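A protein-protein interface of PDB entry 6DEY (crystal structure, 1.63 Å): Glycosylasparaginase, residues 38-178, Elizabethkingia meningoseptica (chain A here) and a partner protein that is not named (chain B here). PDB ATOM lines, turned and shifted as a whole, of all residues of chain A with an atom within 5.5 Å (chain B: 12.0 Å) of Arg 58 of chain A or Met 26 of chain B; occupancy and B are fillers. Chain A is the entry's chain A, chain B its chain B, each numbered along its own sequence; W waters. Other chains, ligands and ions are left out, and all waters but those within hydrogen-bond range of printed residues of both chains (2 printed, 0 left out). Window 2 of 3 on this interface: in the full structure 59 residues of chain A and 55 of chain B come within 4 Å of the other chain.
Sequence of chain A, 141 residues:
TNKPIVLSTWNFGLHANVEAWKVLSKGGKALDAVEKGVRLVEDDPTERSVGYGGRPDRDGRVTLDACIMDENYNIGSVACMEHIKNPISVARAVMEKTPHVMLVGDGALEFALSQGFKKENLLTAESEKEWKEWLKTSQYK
Hydrophobic or aromatic side chains of chain A within 4 Å of the printed part of chain B: Trp 131 and Trp 134.
Along chain A the printed residues that touch a printed residue of chain B span positions 56 to 134.
Hydrophobic or aromatic side chains of chain B that line the printed part of chain A: Tyr 24, Met 26 and His 27.
Among the printed residues, no Asp or Glu carboxylate lies within 4 Å of a Lys or Arg side-chain nitrogen of the other chain.
The backbone carbonyl oxygen of Pro 56 of chain A lies within hydrogen-bond range of the backbone NH of Tyr 24 of chain B, at 2.8 Å.
The backbone NH (N) of Arg 58 of chain A lies within hydrogen-bond range of the backbone carbonyl oxygen (O) of Lys 25 of chain B (2.8 Å).
The side-chain carboxylate (OD2) of Asp 57 of chain A is in hydrogen-bond range of a ring nitrogen (ND1) of His 27 of chain B, at 2.6 Å.
Met 26 of chain B touches just one residue of chain A: Arg 58 (3.8 Å).
No residue of chain B comes within 4 Å of Gly 60 of chain A.
Of the printed residues of chain A, Tyr 24 of chain B touches Pro 56, Asp 57, Arg 58, Trp 131 and Trp 134.
Of the printed residues of chain B, Trp 134 of chain A touches Tyr 24.
The nearest residue of chain B that does not touch Arg 58 of chain A is His 27 of chain B (4.6 Å).
The nearest printed residue of chain B that does not touch Trp 131 of chain A is Ala 23 of chain B (7.5 Å).
Water W1 lies within hydrogen-bond range of OD2 of Asp 57 of chain A (2.7 Å), N of Gly 28 of chain B (2.9 Å) and ND1 of His 27 of chain B (3.4 Å).
Water W2 lies within hydrogen-bond range of OD2 of Asp 59 of chain A, NE of Arg 58 of chain A and N of His 27 of chain B.
OD1 of Asp 57 of chain A is in hydrogen-bond range of N of Asp 59 of chain A, at 2.8 Å.
NE of Arg 58 of chain A lies within hydrogen-bond range of OH of Tyr 140 of chain A, at 3.3 Å.
The side-chain carboxylate of Asp 57 of chain A lies within hydrogen-bond range of the backbone NH of Gly 60 of chain A (3.2 Å).
The backbone carbonyl oxygen of Arg 58 of chain A sits at hydrogen-bond distance from the indole nitrogen of Trp 131 of chain A, 3.0 Å away.
O of Ser 20 of chain B lies within hydrogen-bond range of NZ of Lys 25 of chain B (2.8 Å).
OD1 of Asp 59 of chain A is in hydrogen-bond range of OH of Tyr 140 of chain A (2.6 Å).
C of Ala 23 of chain B touches O of Pro 56 of chain A, at 3.9 Å.
CA of Tyr 24 of chain B touches C of Asp 57 of chain A, 3.8 Å away.
Asp 57 of chain A touches Lys 25 of chain B.
Arg 58 of chain A touches Tyr 24 of chain B (CB to O, 3.5 Å).
Arg 58 of chain A touches Met 26 of chain B (CZ to CG, 3.8 Å).
CB of His 27 of chain B touches OD2 of Asp 59 of chain A (3.5 Å).
Trp 131 of chain A touches Tyr 24 of chain B (N to OH, 3.6 Å).
Tyr 24 of chain B touches Trp 134 of chain A (CD2 to CG, 3.5 Å).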
ATOM      1  N   PRO A  56     -33.419   8.411  24.895  1.00  0.00           N
ATOM      2  CA  PRO A  56     -33.130   6.989  25.036  1.00  0.00           C
ATOM      3  C   PRO A  56     -31.656   6.712  25.155  1.00  0.00           C
ATOM      4  O   PRO A  56     -30.813   7.574  24.884  1.00  0.00           O
ATOM      5  CB  PRO A  56     -33.787   6.363  23.798  1.00  0.00           C
ATOM      6  CG  PRO A  56     -33.656   7.472  22.819  1.00  0.00           C
ATOM      7  CD  PRO A  56     -33.974   8.729  23.557  1.00  0.00           C
ATOM      8  N   ASP A  57     -31.355   5.487  25.498  1.00  0.00           N
ATOM      9  CA  ASP A  57     -30.060   4.877  25.322  1.00  0.00           C
ATOM     10  C   ASP A  57     -29.707   4.708  23.843  1.00  0.00           C
ATOM     11  O   ASP A  57     -30.493   5.122  22.984  1.00  0.00           O
ATOM     12  CB  ASP A  57     -29.908   3.607  26.178  1.00  0.00           C
ATOM     13  CG  ASP A  57     -30.628   2.375  25.672  1.00  0.00           C
ATOM     14  OD1 ASP A  57     -30.997   2.377  24.425  1.00  0.00           O
ATOM     15  OD2 ASP A  57     -30.816   1.434  26.518  1.00  0.00           O
ATOM     16  N   ARG A  58     -28.485   4.252  23.601  1.00  0.00           N
ATOM     17  CA  ARG A  58     -28.004   4.293  22.190  1.00  0.00           C
ATOM     18  C   ARG A  58     -28.827   3.320  21.388  1.00  0.00           C
ATOM     19  O   ARG A  58     -28.787   3.403  20.127  1.00  0.00           O
ATOM     20  CB  ARG A  58     -26.503   4.083  22.115  1.00  0.00           C
ATOM     21  CG  ARG A  58     -26.042   2.707  22.618  1.00  0.00           C
ATOM     22  CD  ARG A  58     -24.551   2.713  22.674  1.00  0.00           C
ATOM     23  NE  ARG A  58     -24.093   1.386  22.941  1.00  0.00           N
ATOM     24  CZ  ARG A  58     -22.809   1.011  22.814  1.00  0.00           C
ATOM     25  NH1 ARG A  58     -21.860   1.873  22.433  1.00  0.00           N
ATOM     26  NH2 ARG A  58     -22.502  -0.231  23.082  1.00  0.00           N
ATOM     27  N   ASP A  59     -29.523   2.360  22.005  1.00  0.00           N
ATOM     28  CA  ASP A  59     -30.357   1.381  21.286  1.00  0.00           C
ATOM     29  C   ASP A  59     -31.836   1.780  21.160  1.00  0.00           C
ATOM     30  O   ASP A  59     -32.647   1.012  20.715  1.00  0.00           O
ATOM     31  CB  ASP A  59     -30.203   0.031  21.931  1.00  0.00           C
ATOM     32  CG  ASP A  59     -28.785  -0.434  21.909  1.00  0.00           C
ATOM     33  OD1 ASP A  59     -28.071  -0.257  20.915  1.00  0.00           O
ATOM     34  OD2 ASP A  59     -28.324  -0.902  22.944  1.00  0.00           O
ATOM     35  N   GLY A  60     -32.118   3.031  21.514  1.00  0.00           N
ATOM     36  CA  GLY A  60     -33.456   3.581  21.418  1.00  0.00           C
ATOM     37  C   GLY A  60     -34.412   3.223  22.504  1.00  0.00           C
ATOM     38  O   GLY A  60     -35.587   3.495  22.361  1.00  0.00           O
ATOM     39  N   TRP A 131     -32.926  10.759  18.416  1.00  0.00           N
ATOM     40  CA  TRP A 131     -32.145   9.544  18.519  1.00  0.00           C
ATOM     41  C   TRP A 131     -31.682   9.139  17.133  1.00  0.00           C
ATOM     42  O   TRP A 131     -30.466   8.955  16.937  1.00  0.00           O
ATOM     43  CB  TRP A 131     -32.895   8.417  19.212  1.00  0.00           C
ATOM     44  CG  TRP A 131     -32.214   7.121  19.129  1.00  0.00           C
ATOM     45  CD1 TRP A 131     -30.968   6.831  19.584  1.00  0.00           C
ATOM     46  CD2 TRP A 131     -32.750   5.917  18.623  1.00  0.00           C
ATOM     47  NE1 TRP A 131     -30.674   5.554  19.336  1.00  0.00           N
ATOM     48  CE2 TRP A 131     -31.758   4.938  18.752  1.00  0.00           C
ATOM     49  CE3 TRP A 131     -33.959   5.572  18.028  1.00  0.00           C
ATOM     50  CZ2 TRP A 131     -31.953   3.616  18.316  1.00  0.00           C
ATOM     51  CZ3 TRP A 131     -34.149   4.270  17.606  1.00  0.00           C
ATOM     52  CH2 TRP A 131     -33.165   3.298  17.762  1.00  0.00           C
ATOM     53  N   TRP A 134     -28.915  11.236  16.011  1.00  0.00           N
ATOM     54  CA  TRP A 134     -27.649  10.852  16.637  1.00  0.00           C
ATOM     55  C   TRP A 134     -27.047   9.597  16.006  1.00  0.00           C
ATOM     56  O   TRP A 134     -25.838   9.476  15.954  1.00  0.00           O
ATOM     57  CB  TRP A 134     -27.857  10.726  18.174  1.00  0.00           C
ATOM     58  CG  TRP A 134     -26.598  10.297  18.904  1.00  0.00           C
ATOM     59  CD1 TRP A 134     -25.618  11.070  19.404  1.00  0.00           C
ATOM     60  CD2 TRP A 134     -26.289   8.971  19.254  1.00  0.00           C
ATOM     61  NE1 TRP A 134     -24.670  10.294  19.986  1.00  0.00           N
ATOM     62  CE2 TRP A 134     -25.048   8.991  19.876  1.00  0.00           C
ATOM     63  CE3 TRP A 134     -26.912   7.754  19.034  1.00  0.00           C
ATOM     64  CZ2 TRP A 134     -24.445   7.788  20.387  1.00  0.00           C
ATOM     65  CZ3 TRP A 134     -26.292   6.594  19.416  1.00  0.00           C
ATOM     66  CH2 TRP A 134     -25.082   6.618  20.094  1.00  0.00           C
ATOM     67  N   LEU A 135     -27.865   8.638  15.620  1.00  0.00           N
ATOM     68  CA  LEU A 135     -27.369   7.403  15.000  1.00  0.00           C
ATOM     69  C   LEU A 135     -26.542   7.773  13.764  1.00  0.00           C
ATOM     70  O   LEU A 135     -25.471   7.174  13.528  1.00  0.00           O
ATOM     71  CB  LEU A 135     -28.457   6.418  14.605  1.00  0.00           C
ATOM     72  CG  LEU A 135     -29.110   5.578  15.720  1.00  0.00           C
ATOM     73  CD1 LEU A 135     -30.305   4.816  15.173  1.00  0.00           C
ATOM     74  CD2 LEU A 135     -28.103   4.608  16.371  1.00  0.00           C
ATOM     75  N   TYR A 140     -23.159   5.158  15.291  1.00  0.00           N
ATOM     76  CA  TYR A 140     -23.278   3.962  16.109  1.00  0.00           C
ATOM     77  C   TYR A 140     -24.209   2.999  15.410  1.00  0.00           C
ATOM     78  O   TYR A 140     -25.166   3.446  14.802  1.00  0.00           O
ATOM     79  CB  TYR A 140     -23.875   4.316  17.485  1.00  0.00           C
ATOM     80  CG  TYR A 140     -24.297   3.095  18.286  1.00  0.00           C
ATOM     81  CD1 TYR A 140     -23.342   2.213  18.829  1.00  0.00           C
ATOM     82  CD2 TYR A 140     -25.685   2.823  18.520  1.00  0.00           C
ATOM     83  CE1 TYR A 140     -23.758   1.074  19.533  1.00  0.00           C
ATOM     84  CE2 TYR A 140     -26.094   1.695  19.216  1.00  0.00           C
ATOM     85  CZ  TYR A 140     -25.124   0.834  19.757  1.00  0.00           C
ATOM     86  OH  TYR A 140     -25.533  -0.277  20.460  1.00  0.00           O
ATOM     87  N   THR B  19     -34.536  10.181  36.880  1.00  0.00           N
ATOM     88  CA  THR B  19     -33.847  10.560  35.672  1.00  0.00           C
ATOM     89  C   THR B  19     -34.086   9.566  34.546  1.00  0.00           C
ATOM     90  O   THR B  19     -34.420   8.386  34.816  1.00  0.00           O
ATOM     91  CB  THR B  19     -32.318  10.676  35.893  1.00  0.00           C
ATOM     92  OG1 THR B  19     -31.674  11.336  34.784  1.00  0.00           O
ATOM     93  CG2 THR B  19     -31.737   9.345  36.182  1.00  0.00           C
ATOM     94  N   SER B  20     -33.884  10.079  33.305  1.00  0.00           N
ATOM     95  CA  SER B  20     -33.678   9.165  32.134  1.00  0.00           C
ATOM     96  C   SER B  20     -32.237   8.894  31.820  1.00  0.00           C
ATOM     97  O   SER B  20     -31.933   8.124  30.926  1.00  0.00           O
ATOM     98  CB  SER B  20     -34.482   9.698  30.933  1.00  0.00           C
ATOM     99  OG  SER B  20     -34.083  10.990  30.558  1.00  0.00           O
ATOM    100  N   GLY B  21     -31.338   9.515  32.594  1.00  0.00           N
ATOM    101  CA  GLY B  21     -29.916   9.207  32.439  1.00  0.00           C
ATOM    102  C   GLY B  21     -29.308   9.900  31.272  1.00  0.00           C
ATOM    103  O   GLY B  21     -29.962  10.676  30.614  1.00  0.00           O
ATOM    104  N   MET B  22     -28.024   9.667  31.050  1.00  0.00           N
ATOM    105  CA  MET B  22     -27.242  10.237  29.965  1.00  0.00           C
ATOM    106  C   MET B  22     -27.797   9.814  28.617  1.00  0.00           C
ATOM    107  O   MET B  22     -28.046   8.600  28.356  1.00  0.00           O
ATOM    108  CB  MET B  22     -25.796   9.795  30.072  1.00  0.00           C
ATOM    109  CG  MET B  22     -25.006  10.228  28.861  1.00  0.00           C
ATOM    110  SD  MET B  22     -23.412   9.464  28.883  1.00  0.00           S
ATOM    111  CE  MET B  22     -22.682  10.428  30.249  1.00  0.00           C
ATOM    112  N   ALA B  23     -28.091  10.820  27.772  1.00  0.00           N
ATOM    113  CA  ALA B  23     -28.614  10.485  26.473  1.00  0.00           C
ATOM    114  C   ALA B  23     -27.639   9.603  25.732  1.00  0.00           C
ATOM    115  O   ALA B  23     -26.463   9.835  25.734  1.00  0.00           O
ATOM    116  CB  ALA B  23     -28.798  11.779  25.668  1.00  0.00           C
ATOM    117  N   TYR B  24     -28.173   8.598  25.094  1.00  0.00           N
ATOM    118  CA  TYR B  24     -27.400   7.667  24.248  1.00  0.00           C
ATOM    119  C   TYR B  24     -26.315   6.865  24.959  1.00  0.00           C
ATOM    120  O   TYR B  24     -25.272   6.473  24.405  1.00  0.00           O
ATOM    121  CB  TYR B  24     -26.892   8.418  22.954  1.00  0.00           C
ATOM    122  CG  TYR B  24     -27.970   9.393  22.392  1.00  0.00           C
ATOM    123  CD1 TYR B  24     -29.231   8.953  22.152  1.00  0.00           C
ATOM    124  CD2 TYR B  24     -27.718  10.726  22.233  1.00  0.00           C
ATOM    125  CE1 TYR B  24     -30.283   9.835  21.780  1.00  0.00           C
ATOM    126  CE2 TYR B  24     -28.715  11.602  21.765  1.00  0.00           C
ATOM    127  CZ  TYR B  24     -29.984  11.140  21.565  1.00  0.00           C
ATOM    128  OH  TYR B  24     -30.985  11.985  21.188  1.00  0.00           O
ATOM    129  N   LYS B  25     -26.516   6.711  26.286  1.00  0.00           N
ATOM    130  CA  LYS B  25     -25.705   5.796  27.063  1.00  0.00           C
ATOM    131  C   LYS B  25     -25.771   4.370  26.469  1.00  0.00           C
ATOM    132  O   LYS B  25     -26.691   3.963  25.782  1.00  0.00           O
ATOM    133  CB  LYS B  25     -26.310   5.745  28.534  1.00  0.00           C
ATOM    134  CG  LYS B  25     -27.746   5.245  28.592  1.00  0.00           C
ATOM    135  CD  LYS B  25     -28.524   5.697  29.855  1.00  0.00           C
ATOM    136  CE  LYS B  25     -29.911   5.117  29.899  1.00  0.00           C
ATOM    137  NZ  LYS B  25     -30.718   5.631  31.031  1.00  0.00           N
ATOM    138  N   MET B  26     -24.813   3.566  26.872  1.00  0.00           N
ATOM    139  CA  MET B  26     -24.832   2.168  26.635  1.00  0.00           C
ATOM    140  C   MET B  26     -26.012   1.544  27.300  1.00  0.00           C
ATOM    141  O   MET B  26     -26.435   1.973  28.385  1.00  0.00           O
ATOM    142  CB  MET B  26     -23.597   1.479  27.166  1.00  0.00           C
ATOM    143  CG  MET B  26     -22.322   1.869  26.501  1.00  0.00           C
ATOM    144  SD  MET B  26     -20.850   1.014  27.195  1.00  0.00           S
ATOM    145  CE  MET B  26     -21.299  -0.674  26.901  1.00  0.00           C
ATOM    146  N   HIS B  27     -26.638   0.578  26.670  1.00  0.00           N
ATOM    147  CA  HIS B  27     -27.772  -0.087  27.313  1.00  0.00           C
ATOM    148  C   HIS B  27     -27.351  -0.720  28.695  1.00  0.00           C
ATOM    149  O   HIS B  27     -26.316  -1.319  28.795  1.00  0.00           O
ATOM    150  CB  HIS B  27     -28.400  -1.190  26.417  1.00  0.00           C
ATOM    151  CG  HIS B  27     -29.601  -1.811  27.042  1.00  0.00           C
ATOM    152  ND1 HIS B  27     -30.793  -1.116  27.155  1.00  0.00           N
ATOM    153  CD2 HIS B  27     -29.858  -3.064  27.454  1.00  0.00           C
ATOM    154  CE1 HIS B  27     -31.702  -1.895  27.721  1.00  0.00           C
ATOM    155  NE2 HIS B  27     -31.158  -3.085  27.919  1.00  0.00           N
ATOM    156  N   GLY B  28     -28.168  -0.444  29.707  1.00  0.00           N
ATOM    157  CA  GLY B  28     -27.880  -0.911  31.032  1.00  0.00           C
ATOM    158  C   GLY B  28     -27.060   0.048  31.826  1.00  0.00           C
ATOM    159  O   GLY B  28     -26.812  -0.241  33.022  1.00  0.00           O
ATOM    160  N   ARG B  29     -26.643   1.155  31.266  1.00  0.00           N
ATOM    161  CA  ARG B  29     -25.894   2.134  32.092  1.00  0.00           C
ATOM    162  C   ARG B  29     -26.758   2.675  33.219  1.00  0.00           C
ATOM    163  O   ARG B  29     -27.858   3.101  33.029  1.00  0.00           O
ATOM    164  CB  ARG B  29     -25.393   3.261  31.255  1.00  0.00           C
ATOM    165  CG  ARG B  29     -24.644   4.410  31.924  1.00  0.00           C
ATOM    166  CD  ARG B  29     -25.508   5.480  32.478  1.00  0.00           C
ATOM    167  NE  ARG B  29     -24.761   6.654  32.919  1.00  0.00           N
ATOM    168  CZ  ARG B  29     -25.319   7.732  33.393  1.00  0.00           C
ATOM    169  NH1 ARG B  29     -26.651   7.857  33.480  1.00  0.00           N
ATOM    170  NH2 ARG B  29     -24.530   8.765  33.760  1.00  0.00           N
ATOM    171  N   VAL B  30     -26.124   2.740  34.406  1.00  0.00           N
ATOM    172  CA  VAL B  30     -26.809   3.369  35.556  1.00  0.00           C
ATOM    173  C   VAL B  30     -25.849   4.498  36.022  1.00  0.00           C
ATOM    174  O   VAL B  30     -24.645   4.303  36.132  1.00  0.00           O
ATOM    175  CB  VAL B  30     -27.058   2.369  36.661  1.00  0.00           C
ATOM    176  CG1 VAL B  30     -27.578   3.036  37.948  1.00  0.00           C
ATOM    177  CG2 VAL B  30     -28.030   1.286  36.132  1.00  0.00           C
ATOM    178  N   GLY B  31     -26.430   5.634  36.321  1.00  0.00           N
ATOM    179  CA  GLY B  31     -25.734   6.758  36.940  1.00  0.00           C
ATOM    180  C   GLY B  31     -25.990   6.892  38.404  1.00  0.00           C
ATOM    181  O   GLY B  31     -26.307   5.958  39.033  1.00  0.00           O
ATOM    182  N   GLU B  56     -21.364   9.365  36.502  1.00  0.00           N
ATOM    183  CA  GLU B  56     -20.190   8.544  36.796  1.00  0.00           C
ATOM    184  C   GLU B  56     -19.264   9.188  37.881  1.00  0.00           C
ATOM    185  O   GLU B  56     -18.665   8.507  38.739  1.00  0.00           O
ATOM    186  CB  GLU B  56     -19.356   8.345  35.520  1.00  0.00           C
ATOM    187  CG  GLU B  56     -19.936   7.364  34.551  1.00  0.00           C
ATOM    188  CD  GLU B  56     -21.198   7.735  33.782  1.00  0.00           C
ATOM    189  OE1 GLU B  56     -21.644   8.917  33.753  1.00  0.00           O
ATOM    190  OE2 GLU B  56     -21.817   6.760  33.252  1.00  0.00           O
HETATM  191  O   HOH W   1     -30.204   1.565  29.131  1.00  0.00           O
HETATM  192  O   HOH W   2     -25.871  -0.504  24.047  1.00  0.00           O
